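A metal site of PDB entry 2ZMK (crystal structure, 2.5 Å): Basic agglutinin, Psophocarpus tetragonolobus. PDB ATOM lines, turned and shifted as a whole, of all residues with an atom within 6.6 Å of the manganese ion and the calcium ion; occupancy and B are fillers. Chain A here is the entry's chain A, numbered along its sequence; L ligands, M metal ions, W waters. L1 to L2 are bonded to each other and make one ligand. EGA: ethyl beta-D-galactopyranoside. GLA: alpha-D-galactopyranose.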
ATOM      1  N   ASP A  87     -25.405  -2.857  27.890  1.00  0.00           N
ATOM      2  CA  ASP A  87     -24.946  -2.883  26.506  1.00  0.00           C
ATOM      3  C   ASP A  87     -24.733  -4.313  26.001  1.00  0.00           C
ATOM      4  O   ASP A  87     -24.811  -4.574  24.793  1.00  0.00           O
ATOM      5  CB  ASP A  87     -23.648  -2.104  26.370  1.00  0.00           C
ATOM      6  CG  ASP A  87     -23.880  -0.644  26.037  1.00  0.00           C
ATOM      7  OD1 ASP A  87     -24.066   0.157  26.975  1.00  0.00           O
ATOM      8  OD2 ASP A  87     -23.899  -0.298  24.840  1.00  0.00           O
ATOM      9  N   GLY A 104     -19.795   1.062  28.087  1.00  0.00           N
ATOM     10  CA  GLY A 104     -20.763   1.243  27.034  1.00  0.00           C
ATOM     11  C   GLY A 104     -20.673   0.203  25.928  1.00  0.00           C
ATOM     12  O   GLY A 104     -20.476  -0.996  26.189  1.00  0.00           O
ATOM     13  N   GLY A 105     -20.808   0.646  24.688  1.00  0.00           N
ATOM     14  CA  GLY A 105     -20.754  -0.245  23.552  1.00  0.00           C
ATOM     15  C   GLY A 105     -19.417  -0.915  23.334  1.00  0.00           C
ATOM     16  O   GLY A 105     -19.277  -1.743  22.431  1.00  0.00           O
ATOM     17  N   TYR A 106     -18.424  -0.572  24.142  1.00  0.00           N
ATOM     18  CA  TYR A 106     -17.106  -1.187  24.020  1.00  0.00           C
ATOM     19  C   TYR A 106     -16.926  -2.346  25.004  1.00  0.00           C
ATOM     20  O   TYR A 106     -15.863  -2.968  25.064  1.00  0.00           O
ATOM     21  CB  TYR A 106     -16.004  -0.148  24.215  1.00  0.00           C
ATOM     22  CG  TYR A 106     -16.000   0.898  23.135  1.00  0.00           C
ATOM     23  CD1 TYR A 106     -15.814   0.547  21.799  1.00  0.00           C
ATOM     24  CD2 TYR A 106     -16.189   2.238  23.444  1.00  0.00           C
ATOM     25  CE1 TYR A 106     -15.826   1.506  20.789  1.00  0.00           C
ATOM     26  CE2 TYR A 106     -16.203   3.218  22.438  1.00  0.00           C
ATOM     27  CZ  TYR A 106     -16.027   2.838  21.110  1.00  0.00           C
ATOM     28  OH  TYR A 106     -16.053   3.801  20.124  1.00  0.00           O
ATOM     29  N   PHE A 107     -17.975  -2.612  25.769  1.00  0.00           N
ATOM     30  CA  PHE A 107     -18.010  -3.731  26.719  1.00  0.00           C
ATOM     31  C   PHE A 107     -16.892  -3.778  27.756  1.00  0.00           C
ATOM     32  O   PHE A 107     -16.840  -4.712  28.545  1.00  0.00           O
ATOM     33  CB  PHE A 107     -18.010  -5.046  25.944  1.00  0.00           C
ATOM     34  CG  PHE A 107     -19.006  -5.109  24.823  1.00  0.00           C
ATOM     35  CD1 PHE A 107     -20.374  -5.128  25.093  1.00  0.00           C
ATOM     36  CD2 PHE A 107     -18.573  -5.183  23.498  1.00  0.00           C
ATOM     37  CE1 PHE A 107     -21.308  -5.224  24.048  1.00  0.00           C
ATOM     38  CE2 PHE A 107     -19.492  -5.276  22.461  1.00  0.00           C
ATOM     39  CZ  PHE A 107     -20.860  -5.295  22.731  1.00  0.00           C
ATOM     40  N   GLU A 122     -19.332 -11.598  21.306  1.00  0.00           N
ATOM     41  CA  GLU A 122     -20.230 -10.701  22.006  1.00  0.00           C
ATOM     42  C   GLU A 122     -21.693 -11.060  21.884  1.00  0.00           C
ATOM     43  O   GLU A 122     -22.130 -11.679  20.911  1.00  0.00           O
ATOM     44  CB  GLU A 122     -20.063  -9.273  21.467  1.00  0.00           C
ATOM     45  CG  GLU A 122     -20.430  -9.180  20.004  1.00  0.00           C
ATOM     46  CD  GLU A 122     -20.451  -7.759  19.479  1.00  0.00           C
ATOM     47  OE1 GLU A 122     -19.424  -7.061  19.577  1.00  0.00           O
ATOM     48  OE2 GLU A 122     -21.512  -7.359  18.967  1.00  0.00           O
ATOM     49  N   ASP A 124     -24.498  -8.745  22.060  1.00  0.00           N
ATOM     50  CA  ASP A 124     -24.830  -7.343  21.984  1.00  0.00           C
ATOM     51  C   ASP A 124     -26.302  -7.033  22.114  1.00  0.00           C
ATOM     52  O   ASP A 124     -27.121  -7.553  21.355  1.00  0.00           O
ATOM     53  CB  ASP A 124     -24.318  -6.787  20.670  1.00  0.00           C
ATOM     54  CG  ASP A 124     -23.975  -5.339  20.771  1.00  0.00           C
ATOM     55  OD1 ASP A 124     -24.653  -4.629  21.541  1.00  0.00           O
ATOM     56  OD2 ASP A 124     -23.020  -4.921  20.092  1.00  0.00           O
ATOM     57  N   THR A 125     -26.634  -6.147  23.044  1.00  0.00           N
ATOM     58  CA  THR A 125     -28.018  -5.809  23.296  1.00  0.00           C
ATOM     59  C   THR A 125     -28.428  -4.370  22.952  1.00  0.00           C
ATOM     60  O   THR A 125     -29.616  -4.059  22.935  1.00  0.00           O
ATOM     61  CB  THR A 125     -28.354  -6.062  24.773  1.00  0.00           C
ATOM     62  OG1 THR A 125     -27.466  -5.304  25.601  1.00  0.00           O
ATOM     63  CG2 THR A 125     -28.206  -7.528  25.091  1.00  0.00           C
ATOM     64  N   PHE A 126     -27.454  -3.506  22.676  1.00  0.00           N
ATOM     65  CA  PHE A 126     -27.744  -2.129  22.330  1.00  0.00           C
ATOM     66  C   PHE A 126     -27.224  -1.832  20.939  1.00  0.00           C
ATOM     67  O   PHE A 126     -26.098  -2.183  20.610  1.00  0.00           O
ATOM     68  CB  PHE A 126     -27.060  -1.179  23.313  1.00  0.00           C
ATOM     69  CG  PHE A 126     -27.288   0.256  22.995  1.00  0.00           C
ATOM     70  CD1 PHE A 126     -28.530   0.839  23.242  1.00  0.00           C
ATOM     71  CD2 PHE A 126     -26.285   1.026  22.419  1.00  0.00           C
ATOM     72  CE1 PHE A 126     -28.767   2.169  22.918  1.00  0.00           C
ATOM     73  CE2 PHE A 126     -26.510   2.362  22.094  1.00  0.00           C
ATOM     74  CZ  PHE A 126     -27.756   2.936  22.340  1.00  0.00           C
ATOM     75  N   ARG A 127     -28.026  -1.164  20.113  1.00  0.00           N
ATOM     76  CA  ARG A 127     -27.574  -0.874  18.765  1.00  0.00           C
ATOM     77  C   ARG A 127     -26.796   0.423  18.602  1.00  0.00           C
ATOM     78  O   ARG A 127     -27.375   1.513  18.571  1.00  0.00           O
ATOM     79  CB  ARG A 127     -28.763  -0.880  17.794  1.00  0.00           C
ATOM     80  CG  ARG A 127     -28.331  -0.693  16.359  1.00  0.00           C
ATOM     81  CD  ARG A 127     -29.461  -0.908  15.383  1.00  0.00           C
ATOM     82  NE  ARG A 127     -28.970  -0.883  14.001  1.00  0.00           N
ATOM     83  CZ  ARG A 127     -29.734  -1.126  12.939  1.00  0.00           C
ATOM     84  NH1 ARG A 127     -31.017  -1.412  13.095  1.00  0.00           N
ATOM     85  NH2 ARG A 127     -29.206  -1.088  11.719  1.00  0.00           N
ATOM     86  N   ASN A 128     -25.476   0.308  18.483  1.00  0.00           N
ATOM     87  CA  ASN A 128     -24.630   1.472  18.273  1.00  0.00           C
ATOM     88  C   ASN A 128     -24.638   1.764  16.776  1.00  0.00           C
ATOM     89  O   ASN A 128     -25.249   1.026  16.001  1.00  0.00           O
ATOM     90  CB  ASN A 128     -23.195   1.199  18.746  1.00  0.00           C
ATOM     91  CG  ASN A 128     -23.084   1.211  20.255  1.00  0.00           C
ATOM     92  OD1 ASN A 128     -23.579   0.314  20.928  1.00  0.00           O
ATOM     93  ND2 ASN A 128     -22.454   2.257  20.800  1.00  0.00           N
ATOM     94  N   TRP A 130     -22.352   1.379  14.617  1.00  0.00           N
ATOM     95  CA  TRP A 130     -21.664   0.324  13.868  1.00  0.00           C
ATOM     96  C   TRP A 130     -22.350  -1.049  13.949  1.00  0.00           C
ATOM     97  O   TRP A 130     -21.831  -2.040  13.430  1.00  0.00           O
ATOM     98  CB  TRP A 130     -20.232   0.201  14.398  1.00  0.00           C
ATOM     99  CG  TRP A 130     -20.185  -0.137  15.859  1.00  0.00           C
ATOM    100  CD1 TRP A 130     -20.467  -1.345  16.428  1.00  0.00           C
ATOM    101  CD2 TRP A 130     -19.900   0.756  16.930  1.00  0.00           C
ATOM    102  NE1 TRP A 130     -20.364  -1.263  17.796  1.00  0.00           N
ATOM    103  CE2 TRP A 130     -20.014   0.019  18.136  1.00  0.00           C
ATOM    104  CE3 TRP A 130     -19.543   2.113  17.013  1.00  0.00           C
ATOM    105  CZ2 TRP A 130     -19.791   0.585  19.389  1.00  0.00           C
ATOM    106  CZ3 TRP A 130     -19.320   2.679  18.266  1.00  0.00           C
ATOM    107  CH2 TRP A 130     -19.443   1.915  19.438  1.00  0.00           C
ATOM    108  N   ASP A 131     -23.518  -1.089  14.590  1.00  0.00           N
ATOM    109  CA  ASP A 131     -24.248  -2.333  14.774  1.00  0.00           C
ATOM    110  C   ASP A 131     -25.446  -2.594  13.906  1.00  0.00           C
ATOM    111  O   ASP A 131     -26.095  -1.663  13.427  1.00  0.00           O
ATOM    112  CB  ASP A 131     -24.809  -2.453  16.204  1.00  0.00           C
ATOM    113  CG  ASP A 131     -23.770  -2.770  17.230  1.00  0.00           C
ATOM    114  OD1 ASP A 131     -22.868  -3.598  16.945  1.00  0.00           O
ATOM    115  OD2 ASP A 131     -23.879  -2.213  18.329  1.00  0.00           O
ATOM    116  N   PRO A 132     -25.752  -3.872  13.682  1.00  0.00           N
ATOM    117  CA  PRO A 132     -26.899  -4.304  12.888  1.00  0.00           C
ATOM    118  C   PRO A 132     -27.985  -4.473  13.956  1.00  0.00           C
ATOM    119  O   PRO A 132     -27.759  -4.140  15.116  1.00  0.00           O
ATOM    120  CB  PRO A 132     -26.434  -5.638  12.310  1.00  0.00           C
ATOM    121  CG  PRO A 132     -25.559  -6.174  13.381  1.00  0.00           C
ATOM    122  CD  PRO A 132     -24.756  -4.960  13.777  1.00  0.00           C
ATOM    123  N   ILE A 134     -30.381  -5.588  16.941  1.00  0.00           N
ATOM    124  CA  ILE A 134     -30.030  -6.223  18.199  1.00  0.00           C
ATOM    125  C   ILE A 134     -31.265  -6.946  18.746  1.00  0.00           C
ATOM    126  O   ILE A 134     -32.391  -6.619  18.389  1.00  0.00           O
ATOM    127  CB  ILE A 134     -29.484  -5.200  19.263  1.00  0.00           C
ATOM    128  CG1 ILE A 134     -30.424  -3.995  19.414  1.00  0.00           C
ATOM    129  CG2 ILE A 134     -28.103  -4.738  18.870  1.00  0.00           C
ATOM    130  CD1 ILE A 134     -31.692  -4.260  20.232  1.00  0.00           C
ATOM    131  N   HIS A 136     -27.769  -9.415  19.072  1.00  0.00           N
ATOM    132  CA  HIS A 136     -27.065 -10.226  18.094  1.00  0.00           C
ATOM    133  C   HIS A 136     -25.782 -10.803  18.667  1.00  0.00           C
ATOM    134  O   HIS A 136     -25.211 -10.248  19.613  1.00  0.00           O
ATOM    135  CB  HIS A 136     -26.752  -9.426  16.829  1.00  0.00           C
ATOM    136  CG  HIS A 136     -25.880  -8.225  17.044  1.00  0.00           C
ATOM    137  ND1 HIS A 136     -26.365  -6.940  16.947  1.00  0.00           N
ATOM    138  CD2 HIS A 136     -24.565  -8.124  17.336  1.00  0.00           C
ATOM    139  CE1 HIS A 136     -25.366  -6.087  17.160  1.00  0.00           C
ATOM    140  NE2 HIS A 136     -24.265  -6.785  17.396  1.00  0.00           N
ATOM    141  N   ILE A 137     -25.370 -11.933  18.123  1.00  0.00           N
ATOM    142  CA  ILE A 137     -24.119 -12.568  18.537  1.00  0.00           C
ATOM    143  C   ILE A 137     -23.137 -12.012  17.536  1.00  0.00           C
ATOM    144  O   ILE A 137     -23.475 -11.838  16.360  1.00  0.00           O
ATOM    145  CB  ILE A 137     -24.132 -14.085  18.360  1.00  0.00           C
ATOM    146  CG1 ILE A 137     -25.337 -14.692  19.055  1.00  0.00           C
ATOM    147  CG2 ILE A 137     -22.872 -14.663  18.937  1.00  0.00           C
ATOM    148  CD1 ILE A 137     -25.480 -16.192  18.824  1.00  0.00           C
ATOM    149  N   GLY A 138     -21.928 -11.717  17.974  1.00  0.00           N
ATOM    150  CA  GLY A 138     -20.950 -11.200  17.059  1.00  0.00           C
ATOM    151  C   GLY A 138     -19.576 -11.745  17.341  1.00  0.00           C
ATOM    152  O   GLY A 138     -19.246 -12.075  18.470  1.00  0.00           O
ATOM    153  N   ASP A 140     -15.801 -10.730  17.275  1.00  0.00           N
ATOM    154  CA  ASP A 140     -14.960  -9.538  17.258  1.00  0.00           C
ATOM    155  C   ASP A 140     -13.473  -9.824  17.274  1.00  0.00           C
ATOM    156  O   ASP A 140     -12.983 -10.597  18.089  1.00  0.00           O
ATOM    157  CB  ASP A 140     -15.280  -8.626  18.448  1.00  0.00           C
ATOM    158  CG  ASP A 140     -16.750  -8.258  18.536  1.00  0.00           C
ATOM    159  OD1 ASP A 140     -17.480  -8.402  17.536  1.00  0.00           O
ATOM    160  OD2 ASP A 140     -17.175  -7.816  19.624  1.00  0.00           O
ATOM    161  N   VAL A 144     -14.823  -3.798  18.027  1.00  0.00           N
ATOM    162  CA  VAL A 144     -16.204  -4.057  18.362  1.00  0.00           C
ATOM    163  C   VAL A 144     -17.054  -4.103  17.092  1.00  0.00           C
ATOM    164  O   VAL A 144     -18.245  -4.397  17.146  1.00  0.00           O
ATOM    165  CB  VAL A 144     -16.703  -2.964  19.349  1.00  0.00           C
ATOM    166  CG1 VAL A 144     -18.198  -2.943  19.413  1.00  0.00           C
ATOM    167  CG2 VAL A 144     -16.139  -3.265  20.738  1.00  0.00           C
ATOM    168  N   ILE A 145     -16.448  -3.811  15.951  1.00  0.00           N
ATOM    169  CA  ILE A 145     -17.188  -3.894  14.695  1.00  0.00           C
ATOM    170  C   ILE A 145     -17.011  -5.335  14.237  1.00  0.00           C
ATOM    171  O   ILE A 145     -16.034  -5.681  13.586  1.00  0.00           O
ATOM    172  CB  ILE A 145     -16.617  -2.918  13.639  1.00  0.00           C
ATOM    173  CG1 ILE A 145     -16.782  -1.475  14.137  1.00  0.00           C
ATOM    174  CG2 ILE A 145     -17.370  -3.077  12.320  1.00  0.00           C
ATOM    175  CD1 ILE A 145     -16.179  -0.447  13.207  1.00  0.00           C
ATOM    176  N   SER A 146     -17.979  -6.176  14.587  1.00  0.00           N
ATOM    177  CA  SER A 146     -17.945  -7.603  14.283  1.00  0.00           C
ATOM    178  C   SER A 146     -17.653  -7.978  12.839  1.00  0.00           C
ATOM    179  O   SER A 146     -18.045  -7.280  11.920  1.00  0.00           O
ATOM    180  CB  SER A 146     -19.279  -8.239  14.698  1.00  0.00           C
ATOM    181  OG  SER A 146     -19.591  -7.888  16.017  1.00  0.00           O
ATOM    182  N   THR A 149     -22.053 -11.515  12.145  1.00  0.00           N
ATOM    183  CA  THR A 149     -23.129 -11.206  13.067  1.00  0.00           C
ATOM    184  C   THR A 149     -24.341 -12.083  12.797  1.00  0.00           C
ATOM    185  O   THR A 149     -24.555 -12.523  11.678  1.00  0.00           O
ATOM    186  CB  THR A 149     -23.531  -9.721  12.894  1.00  0.00           C
ATOM    187  OG1 THR A 149     -23.078  -8.970  14.022  1.00  0.00           O
ATOM    188  CG2 THR A 149     -25.042  -9.564  12.727  1.00  0.00           C
HETATM  189  C2  EGA L   1     -26.502   6.895  21.513  1.00  0.00           C
HETATM  190  C3  EGA L   1     -26.622   7.346  22.987  1.00  0.00           C
HETATM  191  C4  EGA L   1     -25.221   7.425  23.599  1.00  0.00           C
HETATM  192  O5  EGA L   1     -24.278   7.909  21.415  1.00  0.00           O
HETATM  193  C7  EGA L   1     -24.573   8.102  18.510  1.00  0.00           C
HETATM  194  C8  EGA L   1     -25.404   8.512  17.294  1.00  0.00           C
HETATM  195  C1  EGA L   1     -25.569   7.852  20.765  1.00  0.00           C
HETATM  196  C5  EGA L   1     -24.371   8.392  22.776  1.00  0.00           C
HETATM  197  C6  EGA L   1     -22.950   8.553  23.337  1.00  0.00           C
HETATM  198  O1  EGA L   1     -25.405   7.433  19.453  1.00  0.00           O
HETATM  199  O2  EGA L   1     -27.777   6.883  20.898  1.00  0.00           O
HETATM  200  O3  EGA L   1     -27.424   6.443  23.729  1.00  0.00           O
HETATM  201  O4  EGA L   1     -24.614   6.110  23.575  1.00  0.00           O
HETATM  202  O6  EGA L   1     -21.962   8.476  22.317  1.00  0.00           O
HETATM  203  C1  GLA L   2     -24.038   5.691  24.766  1.00  0.00           C
HETATM  204  C2  GLA L   2     -23.134   4.468  24.504  1.00  0.00           C
HETATM  205  C3  GLA L   2     -24.003   3.260  24.101  1.00  0.00           C
HETATM  206  C4  GLA L   2     -25.042   3.005  25.187  1.00  0.00           C
HETATM  207  C5  GLA L   2     -25.892   4.265  25.382  1.00  0.00           C
HETATM  208  C6  GLA L   2     -26.930   4.117  26.476  1.00  0.00           C
HETATM  209  O2  GLA L   2     -22.200   4.764  23.467  1.00  0.00           O
HETATM  210  O3  GLA L   2     -23.181   2.107  23.930  1.00  0.00           O
HETATM  211  O4  GLA L   2     -24.399   2.674  26.411  1.00  0.00           O
HETATM  212  O5  GLA L   2     -25.030   5.370  25.748  1.00  0.00           O
HETATM  213  O6  GLA L   2     -27.755   5.269  26.554  1.00  0.00           O
HETATM  214 MN    MN M   1     -22.495  -5.569  17.926  1.00  0.00          MN
HETATM  215 CA    CA M   2     -23.618  -2.399  20.839  1.00  0.00          CA
HETATM  216  O   HOH W   1     -20.570  -4.712  18.665  1.00  0.00           O
HETATM  217  O   HOH W   2     -20.917  -2.637  20.505  1.00  0.00           O
HETATM  218  O   HOH W   3     -21.194  -6.052  16.054  1.00  0.00           O
HETATM  219  O   HOH W   4     -23.166  -2.351  23.590  1.00  0.00           O
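O of Phe 126 is bound to the calcium ion, 2.5 Å away. The calcium ion is bound by OD2 of Asp 131 (2.5 Å). The calcium ion is bound by the side-chain carboxylate (OD1) of Asp 124 (2.6 Å). OD2 of Asp 124 binds the calcium ion (2.7 Å). The calcium ion is bound by OD1 of Asn 128, 2.7 Å away. Water W2 binds the calcium ion. Water W4 binds the calcium ion (2.8 Å).
The manganese ion is bound by NE2 of His 136 (2.2 Å), water W1 (2.2 Å), OD1 of Asp 131 (2.2 Å), OE2 of Glu 122 (2.3 Å), OD2 of Asp 124 (2.3 Å) and water W3 (2.3 Å). The manganese ion has six donor atoms within binding distance.
N of Gly 105 sits at hydrogen-bond distance from O3 of GLA L2, 2.9 Å away. OD1 of Asp 87 sits at hydrogen-bond distance from O4 of GLA L2 (2.6 Å). The side-chain amide nitrogen (ND2) of Asn 128 sits at hydrogen-bond distance from an oxygen (O3) of GLA L2 (3.2 Å).
The backbone NH (N) of Glu 122 lies within hydrogen-bond range of the backbone carbonyl oxygen (O) of Gly 138. The guanidinium group (NE) of Arg 127 is in hydrogen-bond range of the backbone carbonyl oxygen (O) of Asp 131, 3.0 Å away.
Water W1 bridges the side-chain carboxylate of Glu 122 and the backbone carbonyl oxygen of Val 144. Water W2 bridges O of Gly 105 (2.7 Å) and NE1 of Trp 130 (3.1 Å).
Within 4 Å of the calcium ion: Asp 124, Phe 126, Asn 128 and Asp 131. The nearest printed residue that does not touch the calcium ion is Phe 107 (4.4 Å).
The nearest printed residue that does not touch the manganese ion is Ser 146 (4.2 Å).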
